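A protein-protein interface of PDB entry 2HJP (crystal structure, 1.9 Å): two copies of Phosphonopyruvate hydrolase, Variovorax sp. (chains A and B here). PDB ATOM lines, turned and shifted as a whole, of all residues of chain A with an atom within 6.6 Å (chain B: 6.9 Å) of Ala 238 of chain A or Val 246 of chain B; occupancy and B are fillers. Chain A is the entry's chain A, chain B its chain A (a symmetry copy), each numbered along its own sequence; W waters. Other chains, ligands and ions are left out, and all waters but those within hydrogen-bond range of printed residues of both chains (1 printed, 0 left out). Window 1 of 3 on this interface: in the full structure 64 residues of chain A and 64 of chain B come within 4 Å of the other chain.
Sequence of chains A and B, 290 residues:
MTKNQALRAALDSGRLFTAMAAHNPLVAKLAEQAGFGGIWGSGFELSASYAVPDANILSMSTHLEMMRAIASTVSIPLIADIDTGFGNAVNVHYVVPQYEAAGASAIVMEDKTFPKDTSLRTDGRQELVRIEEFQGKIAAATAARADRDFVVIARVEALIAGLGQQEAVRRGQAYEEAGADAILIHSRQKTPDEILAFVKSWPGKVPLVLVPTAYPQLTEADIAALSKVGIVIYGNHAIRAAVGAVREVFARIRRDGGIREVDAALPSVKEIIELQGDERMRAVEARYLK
The backbone carbonyl oxygen (O) of Tyr 234 of chain A sits at hydrogen-bond distance from the backbone NH (N) of Ala 21 of chain A (3.0 Å). OE2 of Glu 45 of chain A is in hydrogen-bond range of N of Ala 238 of chain A (3.1 Å).
Among the printed residues, merely in contact across the chains: Ala 245 of chain A with Ala 245 of chain B (3.2 Å), Ala 31 of chain A with Phe 250 of chain B (3.3 Å), Val 27 of chain A with Phe 250 of chain B (3.3 Å), Leu 26 of chain A with Val 243 of chain B (3.4 Å), Met 20 of chain A with Phe 250 of chain B (3.4 Å), Ala 34 of chain A with Phe 250 of chain B (3.5 Å), Leu 30 of chain A with Phe 250 of chain B (3.6 Å), Ala 241 of chain A with Val 249 of chain B (3.6 Å), Ala 241 of chain A with Ala 245 of chain B (3.6 Å), Ala 245 of chain A with Ala 241 of chain B (3.6 Å), Ala 238 of chain A with Phe 250 of chain B (3.8 Å), His 237 of chain A with Leu 266 of chain B (3.8 Å), Ala 241 of chain A with Leu 266 of chain B (3.8 Å), Leu 30 of chain A with Val 246 of chain B (3.9 Å), Ala 21 of chain A with Phe 250 of chain B (3.97 Å) and Ala 238 of chain A with Val 246 of chain B (3.99 Å).
Printed residues of chain B within 4 Å of Val 27 of chain A: Phe 250 (3.3 Å). Gly 235 of chain A touches none of the printed residues of chain B. Of the printed residues of chain B, Ala 238 of chain A touches Val 246 and Phe 250. Printed residues of chain B within 4 Å of Ala 241 of chain A: Ala 245 (3.6 Å), Val 249 (3.6 Å) and Leu 266 (3.8 Å). Of the printed residues of chain A, Val 246 of chain B touches Leu 30 and Ala 238.
Printed residues of chain B that touch a printed residue of chain A: Ala 241, Val 243, Ala 245, Val 246, Val 249, Phe 250 and Leu 266. Along chain B the printed residues that touch a printed residue of chain A span positions 241 to 266. Of the 21 printed residues of chain A, 11 touch a printed residue of chain B. Hydrophobic or aromatic side chains of chain A that line the printed part of chain B: Met 20, Leu 26, Val 27, Leu 30, Ala 31, Ala 34, His 237, Ala 238, Ala 241 and Ala 245. Along chain A the printed residues that touch a printed residue of chain B span positions 20 to 245. Among the printed residues, 16 pairs touch across the chains. Among the printed residues, no Asp or Glu carboxylate lies within 4 Å of a Lys or Arg side-chain nitrogen of the other chain.
Ala 241 of chain A touches Ala 245 of chain B, and with the chains exchanged Ala 245 of chain A touches Ala 241 of chain B. Ala 245 of chain A touches its own counterpart, Ala 245 of chain B. Positions printed for both chains: 241, 242, 243 and 245.
Water W1 lies within hydrogen-bond range of O of Leu 266 of chain B and NH2 of Arg 240 of chain A.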
ATOM      1  N   MET A  20       8.633 -36.275  16.152  1.00  0.00           N
ATOM      2  CA  MET A  20       7.502 -35.314  16.354  1.00  0.00           C
ATOM      3  C   MET A  20       6.131 -35.943  16.072  1.00  0.00           C
ATOM      4  O   MET A  20       5.905 -36.692  15.069  1.00  0.00           O
ATOM      5  CB  MET A  20       7.685 -34.111  15.405  1.00  0.00           C
ATOM      6  CG  MET A  20       6.488 -33.107  15.370  1.00  0.00           C
ATOM      7  SD  MET A  20       6.104 -32.479  17.019  1.00  0.00           S
ATOM      8  CE  MET A  20       7.502 -31.309  17.275  1.00  0.00           C
ATOM      9  N   ALA A  21       5.206 -35.610  16.954  1.00  0.00           N
ATOM     10  CA  ALA A  21       3.848 -36.070  16.801  1.00  0.00           C
ATOM     11  C   ALA A  21       3.227 -35.609  15.460  1.00  0.00           C
ATOM     12  O   ALA A  21       3.531 -34.517  14.944  1.00  0.00           O
ATOM     13  CB  ALA A  21       2.998 -35.480  17.953  1.00  0.00           C
ATOM     14  N   ALA A  22       2.326 -36.429  14.922  1.00  0.00           N
ATOM     15  CA  ALA A  22       1.594 -36.073  13.735  1.00  0.00           C
ATOM     16  C   ALA A  22       0.223 -36.726  13.825  1.00  0.00           C
ATOM     17  O   ALA A  22       0.132 -37.888  14.224  1.00  0.00           O
ATOM     18  CB  ALA A  22       2.298 -36.538  12.437  1.00  0.00           C
ATOM     19  N   HIS A  23      -0.834 -35.982  13.477  1.00  0.00           N
ATOM     20  CA  HIS A  23      -2.208 -36.553  13.497  1.00  0.00           C
ATOM     21  C   HIS A  23      -2.708 -36.857  12.051  1.00  0.00           C
ATOM     22  O   HIS A  23      -3.841 -37.351  11.842  1.00  0.00           O
ATOM     23  CB  HIS A  23      -3.188 -35.628  14.268  1.00  0.00           C
ATOM     24  CG  HIS A  23      -3.085 -34.176  13.908  1.00  0.00           C
ATOM     25  ND1 HIS A  23      -2.140 -33.323  14.470  1.00  0.00           N
ATOM     26  CD2 HIS A  23      -3.841 -33.411  13.091  1.00  0.00           C
ATOM     27  CE1 HIS A  23      -2.331 -32.097  14.003  1.00  0.00           C
ATOM     28  NE2 HIS A  23      -3.351 -32.129  13.160  1.00  0.00           N
ATOM     29  N   LEU A  26      -0.104 -34.988   6.219  1.00  0.00           N
ATOM     30  CA  LEU A  26       0.385 -33.655   5.903  1.00  0.00           C
ATOM     31  C   LEU A  26       1.292 -33.145   7.057  1.00  0.00           C
ATOM     32  O   LEU A  26       2.382 -32.636   6.830  1.00  0.00           O
ATOM     33  CB  LEU A  26      -0.791 -32.661   5.603  1.00  0.00           C
ATOM     34  CG  LEU A  26      -0.450 -31.173   5.333  1.00  0.00           C
ATOM     35  CD1 LEU A  26       0.423 -31.056   4.131  1.00  0.00           C
ATOM     36  CD2 LEU A  26      -1.696 -30.311   5.126  1.00  0.00           C
ATOM     37  N   VAL A  27       0.797 -33.237   8.273  1.00  0.00           N
ATOM     38  CA  VAL A  27       1.583 -32.802   9.420  1.00  0.00           C
ATOM     39  C   VAL A  27       2.882 -33.639   9.488  1.00  0.00           C
ATOM     40  O   VAL A  27       3.955 -33.110   9.809  1.00  0.00           O
ATOM     41  CB  VAL A  27       0.768 -33.018  10.727  1.00  0.00           C
ATOM     42  CG1 VAL A  27       1.701 -32.944  11.934  1.00  0.00           C
ATOM     43  CG2 VAL A  27      -0.424 -31.948  10.774  1.00  0.00           C
ATOM     44  N   LEU A  30       5.260 -32.206   7.181  1.00  0.00           N
ATOM     45  CA  LEU A  30       5.895 -30.983   7.637  1.00  0.00           C
ATOM     46  C   LEU A  30       6.990 -31.285   8.653  1.00  0.00           C
ATOM     47  O   LEU A  30       8.016 -30.599   8.655  1.00  0.00           O
ATOM     48  CB  LEU A  30       4.869 -30.011   8.203  1.00  0.00           C
ATOM     49  CG  LEU A  30       3.894 -29.485   7.128  1.00  0.00           C
ATOM     50  CD1 LEU A  30       2.671 -28.847   7.789  1.00  0.00           C
ATOM     51  CD2 LEU A  30       4.616 -28.473   6.202  1.00  0.00           C
ATOM     52  N   ALA A  31       6.759 -32.267   9.529  1.00  0.00           N
ATOM     53  CA  ALA A  31       7.787 -32.641  10.533  1.00  0.00           C
ATOM     54  C   ALA A  31       9.033 -33.106   9.803  1.00  0.00           C
ATOM     55  O   ALA A  31      10.170 -32.708  10.194  1.00  0.00           O
ATOM     56  CB  ALA A  31       7.285 -33.798  11.464  1.00  0.00           C
ATOM     57  N   ALA A  34      10.765 -30.136   8.441  1.00  0.00           N
ATOM     58  CA  ALA A  34      11.369 -29.296   9.515  1.00  0.00           C
ATOM     59  C   ALA A  34      12.697 -29.933  10.004  1.00  0.00           C
ATOM     60  O   ALA A  34      13.485 -29.269  10.631  1.00  0.00           O
ATOM     61  CB  ALA A  34      10.411 -29.119  10.667  1.00  0.00           C
ATOM     62  N   GLU A  45      -2.799 -37.550  19.910  1.00  0.00           N
ATOM     63  CA  GLU A  45      -3.072 -36.654  18.773  1.00  0.00           C
ATOM     64  C   GLU A  45      -4.165 -37.168  17.848  1.00  0.00           C
ATOM     65  O   GLU A  45      -5.037 -36.398  17.462  1.00  0.00           O
ATOM     66  CB  GLU A  45      -1.847 -36.406  17.930  1.00  0.00           C
ATOM     67  CG  GLU A  45      -0.858 -35.428  18.614  1.00  0.00           C
ATOM     68  CD  GLU A  45      -0.373 -34.349  17.670  1.00  0.00           C
ATOM     69  OE1 GLU A  45      -0.665 -34.482  16.448  1.00  0.00           O
ATOM     70  OE2 GLU A  45       0.293 -33.399  18.136  1.00  0.00           O
ATOM     71  N   TYR A 234       8.297 -35.484  20.895  1.00  0.00           N
ATOM     72  CA  TYR A 234       7.432 -34.303  21.126  1.00  0.00           C
ATOM     73  C   TYR A 234       6.044 -34.881  20.972  1.00  0.00           C
ATOM     74  O   TYR A 234       5.543 -35.160  19.866  1.00  0.00           O
ATOM     75  CB  TYR A 234       7.834 -33.234  20.151  1.00  0.00           C
ATOM     76  CG  TYR A 234       9.238 -32.760  20.530  1.00  0.00           C
ATOM     77  CD1 TYR A 234       9.467 -32.152  21.750  1.00  0.00           C
ATOM     78  CD2 TYR A 234      10.322 -32.964  19.672  1.00  0.00           C
ATOM     79  CE1 TYR A 234      10.769 -31.740  22.126  1.00  0.00           C
ATOM     80  CE2 TYR A 234      11.642 -32.561  20.019  1.00  0.00           C
ATOM     81  CZ  TYR A 234      11.834 -31.950  21.263  1.00  0.00           C
ATOM     82  OH  TYR A 234      13.095 -31.577  21.628  1.00  0.00           O
ATOM     83  N   GLY A 235       5.432 -35.078  22.115  1.00  0.00           N
ATOM     84  CA  GLY A 235       4.190 -35.820  22.144  1.00  0.00           C
ATOM     85  C   GLY A 235       2.920 -35.332  21.547  1.00  0.00           C
ATOM     86  O   GLY A 235       2.158 -36.167  21.008  1.00  0.00           O
ATOM     87  N   ASN A 236       2.675 -34.008  21.601  1.00  0.00           N
ATOM     88  CA  ASN A 236       1.377 -33.516  21.097  1.00  0.00           C
ATOM     89  C   ASN A 236       1.374 -32.051  20.643  1.00  0.00           C
ATOM     90  O   ASN A 236       0.336 -31.399  20.636  1.00  0.00           O
ATOM     91  CB  ASN A 236       0.308 -33.714  22.233  1.00  0.00           C
ATOM     92  CG  ASN A 236       0.710 -33.026  23.586  1.00  0.00           C
ATOM     93  OD1 ASN A 236       1.493 -32.091  23.594  1.00  0.00           O
ATOM     94  ND2 ASN A 236       0.152 -33.526  24.725  1.00  0.00           N
ATOM     95  N   HIS A 237       2.518 -31.569  20.187  1.00  0.00           N
ATOM     96  CA  HIS A 237       2.681 -30.191  19.826  1.00  0.00           C
ATOM     97  C   HIS A 237       2.061 -29.847  18.458  1.00  0.00           C
ATOM     98  O   HIS A 237       1.693 -28.675  18.211  1.00  0.00           O
ATOM     99  CB  HIS A 237       4.170 -29.837  19.885  1.00  0.00           C
ATOM    100  CG  HIS A 237       4.788 -30.118  21.220  1.00  0.00           C
ATOM    101  ND1 HIS A 237       5.185 -31.388  21.600  1.00  0.00           N
ATOM    102  CD2 HIS A 237       4.868 -29.341  22.336  1.00  0.00           C
ATOM    103  CE1 HIS A 237       5.465 -31.384  22.903  1.00  0.00           C
ATOM    104  NE2 HIS A 237       5.284 -30.152  23.369  1.00  0.00           N
ATOM    105  N   ALA A 238       1.899 -30.837  17.600  1.00  0.00           N
ATOM    106  CA  ALA A 238       1.263 -30.523  16.302  1.00  0.00           C
ATOM    107  C   ALA A 238      -0.247 -30.285  16.534  1.00  0.00           C
ATOM    108  O   ALA A 238      -0.814 -29.286  16.051  1.00  0.00           O
ATOM    109  CB  ALA A 238       1.412 -31.683  15.329  1.00  0.00           C
ATOM    110  N   ILE A 239      -0.902 -31.155  17.294  1.00  0.00           N
ATOM    111  CA  ILE A 239      -2.364 -30.915  17.412  1.00  0.00           C
ATOM    112  C   ILE A 239      -2.615 -29.582  18.200  1.00  0.00           C
ATOM    113  O   ILE A 239      -3.581 -28.823  17.950  1.00  0.00           O
ATOM    114  CB  ILE A 239      -3.111 -32.164  18.090  1.00  0.00           C
ATOM    115  CG1 ILE A 239      -4.625 -32.029  17.914  1.00  0.00           C
ATOM    116  CG2 ILE A 239      -2.756 -32.277  19.542  1.00  0.00           C
ATOM    117  CD1 ILE A 239      -5.124 -32.265  16.493  1.00  0.00           C
ATOM    118  N   ARG A 240      -1.707 -29.290  19.117  1.00  0.00           N
ATOM    119  CA  ARG A 240      -1.851 -28.106  19.937  1.00  0.00           C
ATOM    120  C   ARG A 240      -1.649 -26.899  19.073  1.00  0.00           C
ATOM    121  O   ARG A 240      -2.479 -25.989  19.119  1.00  0.00           O
ATOM    122  CB  ARG A 240      -0.910 -28.129  21.168  1.00  0.00           C
ATOM    123  CG  ARG A 240      -1.491 -28.983  22.285  1.00  0.00           C
ATOM    124  CD  ARG A 240      -0.336 -29.481  23.251  1.00  0.00           C
ATOM    125  NE  ARG A 240       0.089 -28.386  24.154  1.00  0.00           N
ATOM    126  CZ  ARG A 240       1.239 -28.392  24.803  1.00  0.00           C
ATOM    127  NH1 ARG A 240       2.088 -29.466  24.661  1.00  0.00           N
ATOM    128  NH2 ARG A 240       1.555 -27.311  25.497  1.00  0.00           N
ATOM    129  N   ALA A 241      -0.606 -26.909  18.245  1.00  0.00           N
ATOM    130  CA  ALA A 241      -0.385 -25.785  17.354  1.00  0.00           C
ATOM    131  C   ALA A 241      -1.599 -25.583  16.391  1.00  0.00           C
ATOM    132  O   ALA A 241      -2.014 -24.434  16.088  1.00  0.00           O
ATOM    133  CB  ALA A 241       0.929 -25.989  16.507  1.00  0.00           C
ATOM    134  N   ALA A 242      -2.113 -26.697  15.866  1.00  0.00           N
ATOM    135  CA  ALA A 242      -3.201 -26.658  14.941  1.00  0.00           C
ATOM    136  C   ALA A 242      -4.402 -26.019  15.599  1.00  0.00           C
ATOM    137  O   ALA A 242      -5.018 -25.117  15.026  1.00  0.00           O
ATOM    138  CB  ALA A 242      -3.583 -28.072  14.435  1.00  0.00           C
ATOM    139  N   VAL A 243      -4.758 -26.507  16.789  1.00  0.00           N
ATOM    140  CA  VAL A 243      -5.912 -25.996  17.494  1.00  0.00           C
ATOM    141  C   VAL A 243      -5.765 -24.503  17.743  1.00  0.00           C
ATOM    142  O   VAL A 243      -6.700 -23.734  17.483  1.00  0.00           O
ATOM    143  CB  VAL A 243      -6.164 -26.744  18.862  1.00  0.00           C
ATOM    144  CG1 VAL A 243      -7.081 -25.930  19.771  1.00  0.00           C
ATOM    145  CG2 VAL A 243      -6.802 -28.095  18.616  1.00  0.00           C
ATOM    146  N   ALA A 245      -4.113 -22.274  16.092  1.00  0.00           N
ATOM    147  CA  ALA A 245      -4.295 -21.416  14.920  1.00  0.00           C
ATOM    148  C   ALA A 245      -5.673 -21.500  14.280  1.00  0.00           C
ATOM    149  O   ALA A 245      -6.217 -20.488  13.757  1.00  0.00           O
ATOM    150  CB  ALA A 245      -3.198 -21.680  13.844  1.00  0.00           C
ATOM    151  N   ALA B 241      -4.783 -22.549   7.715  1.00  0.00           N
ATOM    152  CA  ALA B 241      -4.380 -22.067   9.022  1.00  0.00           C
ATOM    153  C   ALA B 241      -3.498 -23.123   9.765  1.00  0.00           C
ATOM    154  O   ALA B 241      -2.503 -22.780  10.454  1.00  0.00           O
ATOM    155  CB  ALA B 241      -5.639 -21.721   9.907  1.00  0.00           C
ATOM    156  N   ALA B 242      -3.910 -24.389   9.671  1.00  0.00           N
ATOM    157  CA  ALA B 242      -3.220 -25.452  10.330  1.00  0.00           C
ATOM    158  C   ALA B 242      -1.800 -25.529   9.818  1.00  0.00           C
ATOM    159  O   ALA B 242      -0.856 -25.588  10.610  1.00  0.00           O
ATOM    160  CB  ALA B 242      -3.919 -26.819  10.113  1.00  0.00           C
ATOM    161  N   VAL B 243      -1.647 -25.561   8.492  1.00  0.00           N
ATOM    162  CA  VAL B 243      -0.336 -25.670   7.892  1.00  0.00           C
ATOM    163  C   VAL B 243       0.547 -24.513   8.332  1.00  0.00           C
ATOM    164  O   VAL B 243       1.698 -24.727   8.736  1.00  0.00           O
ATOM    165  CB  VAL B 243      -0.397 -25.727   6.315  1.00  0.00           C
ATOM    166  CG1 VAL B 243       0.963 -25.403   5.702  1.00  0.00           C
ATOM    167  CG2 VAL B 243      -0.820 -27.105   5.853  1.00  0.00           C
ATOM    168  N   GLY B 244      -0.022 -23.313   8.331  1.00  0.00           N
ATOM    169  CA  GLY B 244       0.756 -22.146   8.697  1.00  0.00           C
ATOM    170  C   GLY B 244       1.285 -22.277  10.094  1.00  0.00           C
ATOM    171  O   GLY B 244       2.481 -22.036  10.306  1.00  0.00           O
ATOM    172  N   ALA B 245       0.454 -22.734  11.024  1.00  0.00           N
ATOM    173  CA  ALA B 245       0.944 -22.799  12.402  1.00  0.00           C
ATOM    174  C   ALA B 245       1.821 -24.005  12.707  1.00  0.00           C
ATOM    175  O   ALA B 245       2.789 -23.926  13.513  1.00  0.00           O
ATOM    176  CB  ALA B 245      -0.227 -22.727  13.428  1.00  0.00           C
ATOM    177  N   VAL B 246       1.513 -25.137  12.076  1.00  0.00           N
ATOM    178  CA  VAL B 246       2.322 -26.344  12.360  1.00  0.00           C
ATOM    179  C   VAL B 246       3.728 -26.179  11.839  1.00  0.00           C
ATOM    180  O   VAL B 246       4.736 -26.515  12.511  1.00  0.00           O
ATOM    181  CB  VAL B 246       1.717 -27.573  11.695  1.00  0.00           C
ATOM    182  CG1 VAL B 246       2.762 -28.737  11.668  1.00  0.00           C
ATOM    183  CG2 VAL B 246       0.429 -27.957  12.495  1.00  0.00           C
ATOM    184  N   ARG B 247       3.794 -25.628  10.633  1.00  0.00           N
ATOM    185  CA  ARG B 247       5.061 -25.368  10.013  1.00  0.00           C
ATOM    186  C   ARG B 247       5.913 -24.403  10.880  1.00  0.00           C
ATOM    187  O   ARG B 247       7.150 -24.566  11.001  1.00  0.00           O
ATOM    188  CB  ARG B 247       4.750 -24.723   8.666  1.00  0.00           C
ATOM    189  CG  ARG B 247       5.760 -24.866   7.695  1.00  0.00           C
ATOM    190  CD  ARG B 247       5.181 -24.362   6.356  1.00  0.00           C
ATOM    191  NE  ARG B 247       4.549 -23.039   6.458  1.00  0.00           N
ATOM    192  CZ  ARG B 247       4.087 -22.378   5.382  1.00  0.00           C
ATOM    193  NH1 ARG B 247       4.192 -22.939   4.160  1.00  0.00           N
ATOM    194  NH2 ARG B 247       3.548 -21.172   5.515  1.00  0.00           N
ATOM    195  N   GLU B 248       5.269 -23.376  11.448  1.00  0.00           N
ATOM    196  CA  GLU B 248       6.004 -22.401  12.250  1.00  0.00           C
ATOM    197  C   GLU B 248       6.457 -23.004  13.590  1.00  0.00           C
ATOM    198  O   GLU B 248       7.602 -22.774  14.025  1.00  0.00           O
ATOM    199  CB  GLU B 248       5.133 -21.131  12.519  1.00  0.00           C
ATOM    200  CG  GLU B 248       5.889 -19.973  13.201  1.00  0.00           C
ATOM    201  N   VAL B 249       5.579 -23.760  14.256  1.00  0.00           N
ATOM    202  CA  VAL B 249       5.951 -24.345  15.524  1.00  0.00           C
ATOM    203  C   VAL B 249       7.099 -25.369  15.279  1.00  0.00           C
ATOM    204  O   VAL B 249       8.035 -25.402  16.041  1.00  0.00           O
ATOM    205  CB  VAL B 249       4.739 -25.020  16.211  1.00  0.00           C
ATOM    206  CG1 VAL B 249       4.331 -26.201  15.437  1.00  0.00           C
ATOM    207  CG2 VAL B 249       5.071 -25.544  17.597  1.00  0.00           C
ATOM    208  N   PHE B 250       7.031 -26.150  14.190  1.00  0.00           N
ATOM    209  CA  PHE B 250       8.063 -27.140  13.915  1.00  0.00           C
ATOM    210  C   PHE B 250       9.395 -26.446  13.674  1.00  0.00           C
ATOM    211  O   PHE B 250      10.452 -26.902  14.168  1.00  0.00           O
ATOM    212  CB  PHE B 250       7.728 -27.998  12.684  1.00  0.00           C
ATOM    213  CG  PHE B 250       6.602 -29.034  12.897  1.00  0.00           C
ATOM    214  CD1 PHE B 250       6.002 -29.214  14.138  1.00  0.00           C
ATOM    215  CD2 PHE B 250       6.195 -29.871  11.822  1.00  0.00           C
ATOM    216  CE1 PHE B 250       4.986 -30.208  14.359  1.00  0.00           C
ATOM    217  CE2 PHE B 250       5.153 -30.902  12.022  1.00  0.00           C
ATOM    218  CZ  PHE B 250       4.557 -31.053  13.289  1.00  0.00           C
ATOM    219  N   ALA B 251       9.350 -25.335  12.943  1.00  0.00           N
ATOM    220  CA  ALA B 251      10.596 -24.609  12.609  1.00  0.00           C
ATOM    221  C   ALA B 251      11.159 -24.010  13.900  1.00  0.00           C
ATOM    222  O   ALA B 251      12.367 -24.028  14.105  1.00  0.00           O
ATOM    223  CB  ALA B 251      10.312 -23.517  11.587  1.00  0.00           C
ATOM    224  N   ARG B 252      10.314 -23.472  14.781  1.00  0.00           N
ATOM    225  CA  ARG B 252      10.810 -22.937  16.038  1.00  0.00           C
ATOM    226  C   ARG B 252      11.426 -24.015  16.928  1.00  0.00           C
ATOM    227  O   ARG B 252      12.504 -23.794  17.533  1.00  0.00           O
ATOM    228  CB  ARG B 252       9.714 -22.228  16.845  1.00  0.00           C
ATOM    229  CG  ARG B 252       9.247 -20.935  16.180  1.00  0.00           C
ATOM    230  CD  ARG B 252       8.075 -20.215  16.870  1.00  0.00           C
ATOM    231  NE  ARG B 252       8.403 -19.784  18.242  1.00  0.00           N
ATOM    232  CZ  ARG B 252       7.496 -19.498  19.196  1.00  0.00           C
ATOM    233  NH1 ARG B 252       6.167 -19.612  18.952  1.00  0.00           N
ATOM    234  NH2 ARG B 252       7.918 -19.065  20.384  1.00  0.00           N
ATOM    235  N   LEU B 266       1.456 -22.117  23.047  1.00  0.00           N
ATOM    236  CA  LEU B 266       0.489 -23.136  22.577  1.00  0.00           C
ATOM    237  C   LEU B 266      -0.787 -23.324  23.418  1.00  0.00           C
ATOM    238  O   LEU B 266      -0.774 -23.091  24.606  1.00  0.00           O
ATOM    239  CB  LEU B 266       1.202 -24.523  22.610  1.00  0.00           C
ATOM    240  CG  LEU B 266       2.368 -24.674  21.633  1.00  0.00           C
ATOM    241  CD1 LEU B 266       3.010 -26.075  21.699  1.00  0.00           C
ATOM    242  CD2 LEU B 266       1.817 -24.442  20.198  1.00  0.00           C
HETATM  243  O   HOH W   1       0.608 -24.619  26.408  1.00  0.00           O
